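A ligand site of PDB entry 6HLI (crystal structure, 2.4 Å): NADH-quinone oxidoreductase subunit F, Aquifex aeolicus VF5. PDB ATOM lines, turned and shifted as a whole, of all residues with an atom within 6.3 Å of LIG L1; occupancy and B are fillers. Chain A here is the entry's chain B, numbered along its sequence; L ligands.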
ATOM      1  N   ILE A 181      28.809 -16.670  31.288  1.00  0.00           N
ATOM      2  CA  ILE A 181      28.124 -17.652  30.460  1.00  0.00           C
ATOM      3  C   ILE A 181      29.009 -18.866  30.114  1.00  0.00           C
ATOM      4  O   ILE A 181      28.469 -19.937  29.836  1.00  0.00           O
ATOM      5  CB  ILE A 181      27.532 -16.943  29.199  1.00  0.00           C
ATOM      6  CG1 ILE A 181      26.381 -17.754  28.524  1.00  0.00           C
ATOM      7  CG2 ILE A 181      28.620 -16.556  28.171  1.00  0.00           C
ATOM      8  CD1 ILE A 181      25.316 -18.241  29.441  1.00  0.00           C
ATOM      9  N   HIS A 198      29.148 -19.130  23.406  1.00  0.00           N
ATOM     10  CA  HIS A 198      27.723 -19.185  23.127  1.00  0.00           C
ATOM     11  C   HIS A 198      27.167 -20.563  23.436  1.00  0.00           C
ATOM     12  O   HIS A 198      27.557 -21.526  22.780  1.00  0.00           O
ATOM     13  CB  HIS A 198      27.401 -18.825  21.664  1.00  0.00           C
ATOM     14  CG  HIS A 198      27.629 -17.404  21.294  1.00  0.00           C
ATOM     15  ND1 HIS A 198      28.459 -17.062  20.249  1.00  0.00           N
ATOM     16  CD2 HIS A 198      27.118 -16.268  21.829  1.00  0.00           C
ATOM     17  CE1 HIS A 198      28.431 -15.743  20.189  1.00  0.00           C
ATOM     18  NE2 HIS A 198      27.649 -15.215  21.127  1.00  0.00           N
ATOM     19  N   PRO A 199      26.197 -20.667  24.373  1.00  0.00           N
ATOM     20  CA  PRO A 199      25.575 -21.980  24.634  1.00  0.00           C
ATOM     21  C   PRO A 199      24.920 -22.562  23.383  1.00  0.00           C
ATOM     22  O   PRO A 199      24.363 -21.822  22.580  1.00  0.00           O
ATOM     23  CB  PRO A 199      24.492 -21.645  25.672  1.00  0.00           C
ATOM     24  CG  PRO A 199      24.962 -20.411  26.319  1.00  0.00           C
ATOM     25  CD  PRO A 199      25.615 -19.625  25.242  1.00  0.00           C
ATOM     26  N   LYS A 202      20.308 -27.533  23.770  1.00  0.00           N
ATOM     27  CA  LYS A 202      20.316 -28.833  24.441  1.00  0.00           C
ATOM     28  C   LYS A 202      18.870 -29.379  24.563  1.00  0.00           C
ATOM     29  O   LYS A 202      18.004 -28.629  25.001  1.00  0.00           O
ATOM     30  CB  LYS A 202      20.969 -28.757  25.820  1.00  0.00           C
ATOM     31  CG  LYS A 202      22.261 -27.971  25.851  1.00  0.00           C
ATOM     32  CD  LYS A 202      22.466 -27.250  27.191  1.00  0.00           C
ATOM     33  CE  LYS A 202      21.655 -25.981  27.349  1.00  0.00           C
ATOM     34  NZ  LYS A 202      22.220 -24.842  26.559  1.00  0.00           N
ATOM     35  N   GLU A 345      25.899 -10.119  31.744  1.00  0.00           N
ATOM     36  CA  GLU A 345      26.273 -11.491  31.421  1.00  0.00           C
ATOM     37  C   GLU A 345      25.496 -12.182  30.290  1.00  0.00           C
ATOM     38  O   GLU A 345      25.925 -13.247  29.856  1.00  0.00           O
ATOM     39  CB  GLU A 345      26.251 -12.372  32.678  1.00  0.00           C
ATOM     40  CG  GLU A 345      27.195 -11.944  33.791  1.00  0.00           C
ATOM     41  CD  GLU A 345      28.592 -11.438  33.482  1.00  0.00           C
ATOM     42  OE1 GLU A 345      29.247 -11.954  32.540  1.00  0.00           O
ATOM     43  OE2 GLU A 345      29.050 -10.540  34.227  1.00  0.00           O
ATOM     44  N   THR A 346      24.373 -11.611  29.810  1.00  0.00           N
ATOM     45  CA  THR A 346      23.615 -12.226  28.712  1.00  0.00           C
ATOM     46  C   THR A 346      24.495 -12.335  27.436  1.00  0.00           C
ATOM     47  O   THR A 346      25.139 -11.345  27.066  1.00  0.00           O
ATOM     48  CB  THR A 346      22.271 -11.526  28.471  1.00  0.00           C
ATOM     49  OG1 THR A 346      21.637 -12.136  27.331  1.00  0.00           O
ATOM     50  CG2 THR A 346      22.418 -10.032  28.246  1.00  0.00           C
ATOM     51  N   CYS A 347      24.548 -13.519  26.790  1.00  0.00           N
ATOM     52  CA  CYS A 347      25.352 -13.624  25.567  1.00  0.00           C
ATOM     53  C   CYS A 347      24.656 -12.950  24.343  1.00  0.00           C
ATOM     54  O   CYS A 347      25.320 -12.644  23.341  1.00  0.00           O
ATOM     55  CB  CYS A 347      25.789 -15.062  25.279  1.00  0.00           C
ATOM     56  SG  CYS A 347      24.480 -16.126  24.647  1.00  0.00           S
ATOM     57  N   GLY A 348      23.349 -12.707  24.477  1.00  0.00           N
ATOM     58  CA  GLY A 348      22.557 -12.005  23.482  1.00  0.00           C
ATOM     59  C   GLY A 348      22.015 -12.829  22.330  1.00  0.00           C
ATOM     60  O   GLY A 348      21.420 -12.262  21.419  1.00  0.00           O
ATOM     61  N   GLN A 349      22.195 -14.157  22.358  1.00  0.00           N
ATOM     62  CA  GLN A 349      21.732 -15.098  21.327  1.00  0.00           C
ATOM     63  C   GLN A 349      20.204 -15.087  21.191  1.00  0.00           C
ATOM     64  O   GLN A 349      19.647 -15.150  20.075  1.00  0.00           O
ATOM     65  CB  GLN A 349      22.183 -16.519  21.665  1.00  0.00           C
ATOM     66  CG  GLN A 349      23.500 -16.946  21.055  1.00  0.00           C
ATOM     67  CD  GLN A 349      23.679 -18.442  21.165  1.00  0.00           C
ATOM     68  OE1 GLN A 349      23.803 -19.150  20.154  1.00  0.00           O
ATOM     69  NE2 GLN A 349      23.691 -18.970  22.388  1.00  0.00           N
ATOM     70  N   CYS A 350      19.540 -15.037  22.364  1.00  0.00           N
ATOM     71  CA  CYS A 350      18.091 -15.069  22.541  1.00  0.00           C
ATOM     72  C   CYS A 350      17.611 -13.638  22.730  1.00  0.00           C
ATOM     73  O   CYS A 350      18.126 -12.944  23.602  1.00  0.00           O
ATOM     74  CB  CYS A 350      17.717 -15.970  23.718  1.00  0.00           C
ATOM     75  SG  CYS A 350      18.544 -17.607  23.703  1.00  0.00           S
ATOM     76  N   THR A 351      16.686 -13.196  21.870  1.00  0.00           N
ATOM     77  CA  THR A 351      16.112 -11.848  21.836  1.00  0.00           C
ATOM     78  C   THR A 351      15.467 -11.470  23.174  1.00  0.00           C
ATOM     79  O   THR A 351      15.832 -10.397  23.660  1.00  0.00           O
ATOM     80  CB  THR A 351      15.175 -11.649  20.610  1.00  0.00           C
ATOM     81  OG1 THR A 351      15.940 -11.811  19.413  1.00  0.00           O
ATOM     82  CG2 THR A 351      14.483 -10.276  20.591  1.00  0.00           C
ATOM     83  N   CYS A 353      16.058 -12.683  26.149  1.00  0.00           N
ATOM     84  CA  CYS A 353      17.116 -12.623  27.133  1.00  0.00           C
ATOM     85  C   CYS A 353      17.978 -11.367  26.911  1.00  0.00           C
ATOM     86  O   CYS A 353      18.245 -10.630  27.874  1.00  0.00           O
ATOM     87  CB  CYS A 353      17.957 -13.893  27.167  1.00  0.00           C
ATOM     88  SG  CYS A 353      19.298 -13.847  28.400  1.00  0.00           S
ATOM     89  N   ARG A 354      18.385 -11.127  25.632  1.00  0.00           N
ATOM     90  CA  ARG A 354      19.189  -9.961  25.240  1.00  0.00           C
ATOM     91  C   ARG A 354      18.541  -8.637  25.719  1.00  0.00           C
ATOM     92  O   ARG A 354      19.185  -7.881  26.464  1.00  0.00           O
ATOM     93  CB  ARG A 354      19.443  -9.963  23.714  1.00  0.00           C
ATOM     94  CG  ARG A 354      20.270  -8.782  23.197  1.00  0.00           C
ATOM     95  CD  ARG A 354      20.541  -8.851  21.687  1.00  0.00           C
ATOM     96  NE  ARG A 354      19.360  -8.585  20.870  1.00  0.00           N
ATOM     97  CZ  ARG A 354      18.685  -9.531  20.218  1.00  0.00           C
ATOM     98  NH1 ARG A 354      19.061 -10.807  20.289  1.00  0.00           N
ATOM     99  NH2 ARG A 354      17.622  -9.210  19.483  1.00  0.00           N
ATOM    100  N   CYS A 357      17.267  -8.686  29.844  1.00  0.00           N
ATOM    101  CA  CYS A 357      18.348  -8.467  30.824  1.00  0.00           C
ATOM    102  C   CYS A 357      18.806  -7.027  30.812  1.00  0.00           C
ATOM    103  O   CYS A 357      19.019  -6.445  31.881  1.00  0.00           O
ATOM    104  CB  CYS A 357      19.500  -9.450  30.621  1.00  0.00           C
ATOM    105  SG  CYS A 357      19.122 -11.152  31.111  1.00  0.00           S
ATOM    106  N   ILE A 387      11.860 -12.787  30.251  1.00  0.00           N
ATOM    107  CA  ILE A 387      13.265 -12.932  29.865  1.00  0.00           C
ATOM    108  C   ILE A 387      13.439 -14.386  29.351  1.00  0.00           C
ATOM    109  O   ILE A 387      14.116 -14.603  28.337  1.00  0.00           O
ATOM    110  CB  ILE A 387      14.267 -12.557  31.026  1.00  0.00           C
ATOM    111  CG1 ILE A 387      14.016 -11.100  31.548  1.00  0.00           C
ATOM    112  CG2 ILE A 387      15.721 -12.719  30.558  1.00  0.00           C
ATOM    113  CD1 ILE A 387      14.768 -10.700  32.833  1.00  0.00           C
ATOM    114  N   THR A 390      11.923 -18.431  24.688  1.00  0.00           N
ATOM    115  CA  THR A 390      12.832 -18.855  23.594  1.00  0.00           C
ATOM    116  C   THR A 390      14.310 -19.086  24.038  1.00  0.00           C
ATOM    117  O   THR A 390      15.140 -19.495  23.193  1.00  0.00           O
ATOM    118  CB  THR A 390      12.750 -17.919  22.343  1.00  0.00           C
ATOM    119  OG1 THR A 390      13.564 -16.757  22.523  1.00  0.00           O
ATOM    120  CG2 THR A 390      11.325 -17.513  21.981  1.00  0.00           C
ATOM    121  N   SER A 391      14.640 -18.865  25.330  1.00  0.00           N
ATOM    122  CA  SER A 391      16.002 -19.023  25.859  1.00  0.00           C
ATOM    123  C   SER A 391      16.503 -20.465  25.705  1.00  0.00           C
ATOM    124  O   SER A 391      15.746 -21.419  25.946  1.00  0.00           O
ATOM    125  CB  SER A 391      16.088 -18.560  27.308  1.00  0.00           C
ATOM    126  OG  SER A 391      15.219 -19.280  28.172  1.00  0.00           O
ATOM    127  N   ILE A 392      17.757 -20.628  25.260  1.00  0.00           N
ATOM    128  CA  ILE A 392      18.336 -21.957  25.054  1.00  0.00           C
ATOM    129  C   ILE A 392      19.238 -22.334  26.209  1.00  0.00           C
ATOM    130  O   ILE A 392      19.676 -23.483  26.281  1.00  0.00           O
ATOM    131  CB  ILE A 392      19.000 -22.161  23.665  1.00  0.00           C
ATOM    132  CG1 ILE A 392      20.152 -21.148  23.378  1.00  0.00           C
ATOM    133  CG2 ILE A 392      17.945 -22.114  22.588  1.00  0.00           C
ATOM    134  CD1 ILE A 392      21.032 -21.480  22.178  1.00  0.00           C
ATOM    135  N   CYS A 393      19.497 -21.398  27.131  1.00  0.00           N
ATOM    136  CA  CYS A 393      20.286 -21.753  28.307  1.00  0.00           C
ATOM    137  C   CYS A 393      19.660 -21.211  29.605  1.00  0.00           C
ATOM    138  O   CYS A 393      18.755 -20.363  29.557  1.00  0.00           O
ATOM    139  CB  CYS A 393      21.758 -21.375  28.158  1.00  0.00           C
ATOM    140  SG  CYS A 393      22.252 -19.845  28.990  1.00  0.00           S
ATOM    141  N   GLY A 394      20.078 -21.787  30.733  1.00  0.00           N
ATOM    142  CA  GLY A 394      19.595 -21.481  32.078  1.00  0.00           C
ATOM    143  C   GLY A 394      19.646 -20.034  32.514  1.00  0.00           C
ATOM    144  O   GLY A 394      18.928 -19.663  33.444  1.00  0.00           O
ATOM    145  N   LEU A 395      20.486 -19.182  31.847  1.00  0.00           N
ATOM    146  CA  LEU A 395      20.621 -17.762  32.166  1.00  0.00           C
ATOM    147  C   LEU A 395      19.315 -16.989  31.970  1.00  0.00           C
ATOM    148  O   LEU A 395      18.900 -16.282  32.891  1.00  0.00           O
ATOM    149  CB  LEU A 395      21.769 -17.086  31.374  1.00  0.00           C
ATOM    150  CG  LEU A 395      22.292 -15.741  31.930  1.00  0.00           C
ATOM    151  CD1 LEU A 395      23.774 -15.570  31.626  1.00  0.00           C
ATOM    152  CD2 LEU A 395      21.464 -14.538  31.420  1.00  0.00           C
ATOM    153  N   GLY A 396      18.716 -17.103  30.770  1.00  0.00           N
ATOM    154  CA  GLY A 396      17.459 -16.444  30.429  1.00  0.00           C
ATOM    155  C   GLY A 396      16.326 -16.921  31.322  1.00  0.00           C
ATOM    156  O   GLY A 396      15.456 -16.131  31.688  1.00  0.00           O
ATOM    157  N   ALA A 397      16.390 -18.218  31.715  1.00  0.00           N
ATOM    158  CA  ALA A 397      15.409 -18.882  32.564  1.00  0.00           C
ATOM    159  C   ALA A 397      15.364 -18.350  33.978  1.00  0.00           C
ATOM    160  O   ALA A 397      14.302 -18.395  34.595  1.00  0.00           O
ATOM    161  CB  ALA A 397      15.671 -20.387  32.598  1.00  0.00           C
HETATM  162 FE1  LIG L   1      22.638 -16.490  25.800  1.00  0.00          FE
HETATM  163 FE2  LIG L   1      20.543 -15.577  27.347  1.00  0.00          FE
HETATM  164 FE3  LIG L   1      21.404 -18.187  27.594  1.00  0.00          FE
HETATM  165 FE4  LIG L   1      20.053 -17.375  25.292  1.00  0.00          FE
HETATM  166  S1  LIG L   1      19.222 -17.493  27.473  1.00  0.00           S
HETATM  167  S2  LIG L   1      21.955 -18.691  25.395  1.00  0.00           S
HETATM  168  S3  LIG L   1      20.873 -15.210  25.093  1.00  0.00           S
HETATM  169  S4  LIG L   1      22.606 -16.266  28.097  1.00  0.00           S
HETATM  170  N1  LG2 L   2      28.802 -24.922  36.759  1.00  0.00           N
HETATM  171  C1  LG2 L   2      30.025 -24.795  37.357  1.00  0.00           C
HETATM  172  O1  LG2 L   2      30.650 -25.781  37.755  1.00  0.00           O
HETATM  173  N2  LG2 L   2      30.644 -23.552  37.418  1.00  0.00           N
HETATM  174  C2  LG2 L   2      30.172 -22.372  36.870  1.00  0.00           C
HETATM  175  O2  LG2 L   2      30.774 -21.326  37.051  1.00  0.00           O
HETATM  176  C3  LG2 L   2      28.901 -22.519  36.169  1.00  0.00           C
HETATM  177  N3  LG2 L   2      28.409 -21.479  35.563  1.00  0.00           N
HETATM  178  C4  LG2 L   2      27.164 -21.606  34.941  1.00  0.00           C
HETATM  179  C5  LG2 L   2      26.613 -20.477  34.324  1.00  0.00           C
HETATM  180  C6  LG2 L   2      25.350 -20.528  33.736  1.00  0.00           C
HETATM  181  C7  LG2 L   2      24.804 -19.300  33.049  1.00  0.00           C
HETATM  182  C8  LG2 L   2      24.619 -21.740  33.760  1.00  0.00           C
HETATM  183  C9  LG2 L   2      23.255 -21.859  33.111  1.00  0.00           C
HETATM  184  C10 LG2 L   2      25.177 -22.872  34.354  1.00  0.00           C
HETATM  185  C11 LG2 L   2      26.440 -22.821  34.942  1.00  0.00           C
HETATM  186  N4  LG2 L   2      27.037 -23.959  35.557  1.00  0.00           N
HETATM  187  C12 LG2 L   2      28.266 -23.844  36.185  1.00  0.00           C
HETATM  188  C13 LG2 L   2      26.397 -25.281  35.419  1.00  0.00           C
HETATM  189  C14 LG2 L   2      26.962 -26.082  34.240  1.00  0.00           C
HETATM  190  O3  LG2 L   2      26.230 -25.781  33.039  1.00  0.00           O
HETATM  191  C15 LG2 L   2      26.956 -27.593  34.496  1.00  0.00           C
HETATM  192  O4  LG2 L   2      25.632 -28.026  34.835  1.00  0.00           O
HETATM  193  C16 LG2 L   2      27.949 -28.105  35.545  1.00  0.00           C
HETATM  194  O5  LG2 L   2      29.268 -27.595  35.318  1.00  0.00           O
HETATM  195  C17 LG2 L   2      27.984 -29.615  35.549  1.00  0.00           C
HETATM  196  O6  LG2 L   2      28.719 -30.109  36.681  1.00  0.00           O
HETATM  197  P1  LG2 L   2      28.028 -30.869  37.924  1.00  0.00           P
HETATM  198  O7  LG2 L   2      27.265 -29.927  38.879  1.00  0.00           O
HETATM  199  O8  LG2 L   2      27.110 -31.962  37.380  1.00  0.00           O
HETATM  200  O9  LG2 L   2      29.194 -31.546  38.633  1.00  0.00           O
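CD1 of Ile 181 touches S4 of LIG L1, 3.6 Å away. Pro 199 touches LIG L1 (CG to S2, 3.6 Å). Thr 346 touches LIG L1. Ser 391 touches LIG L1 (CB to S1, 3.3 Å). Ile 392 touches LIG L1 (CG1 to S2, 3.7 Å). CB of Leu 395 touches S4 of LIG L1 (3.5 Å). Hydrophobic or aromatic side chains that line LIG L1: Ile 181, Pro 199, Ile 392 and Leu 395.
The backbone NH (N) of Leu 395 lies close to the side-chain sulfur (SG) of Cys 393, at 3.4 Å. NE2 of Gln 349 lies close to SG of Cys 347, at 3.7 Å. The guanidinium group of Arg 354 is in hydrogen-bond range of the backbone carbonyl oxygen of Gly 348 (3.0 Å). The backbone carbonyl oxygen (O) of Pro 199 lies within hydrogen-bond range of the side-chain amide nitrogen (NE2) of Gln 349 (2.9 Å). The side-chain hydroxyl of Thr 346 sits close to the backbone NH of Gly 348 (3.4 Å). The side-chain sulfur (SG) of Cys 357 lies close to the backbone carbonyl oxygen (O) of Cys 353 (3.4 Å). The backbone carbonyl oxygen of Ile 392 lies within hydrogen-bond range of the side-chain amino group of Lys 202. The side-chain sulfur (SG) of Cys 350 lies close to the backbone NH (N) of Ile 392.
The side-chain sulfur (SG) of Cys 393 binds an iron atom (FE3) of LIG L1 (2.3 Å). N of Cys 350 lies close to S3 of LIG L1 (3.0 Å). The side-chain amide nitrogen of Gln 349 sits close to a sulfur (S2) of LIG L1, at 3.5 Å. An iron atom (FE4) of LIG L1 is bound by the side-chain sulfur of Cys 350 (2.2 Å). S3 of LIG L1 lies close to N of Gly 348 (3.6 Å). The backbone NH (N) of Cys 347 lies close to a sulfur (S4) of LIG L1 (3.6 Å). The backbone NH (N) of Gln 349 lies close to a sulfur (S3) of LIG L1 (3.2 Å). SG of Cys 347 binds FE1 of LIG L1 (2.2 Å). SG of Cys 353 binds FE2 of LIG L1, 2.4 Å away. S1 of LIG L1 lies close to N of Gly 396 (3.4 Å).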
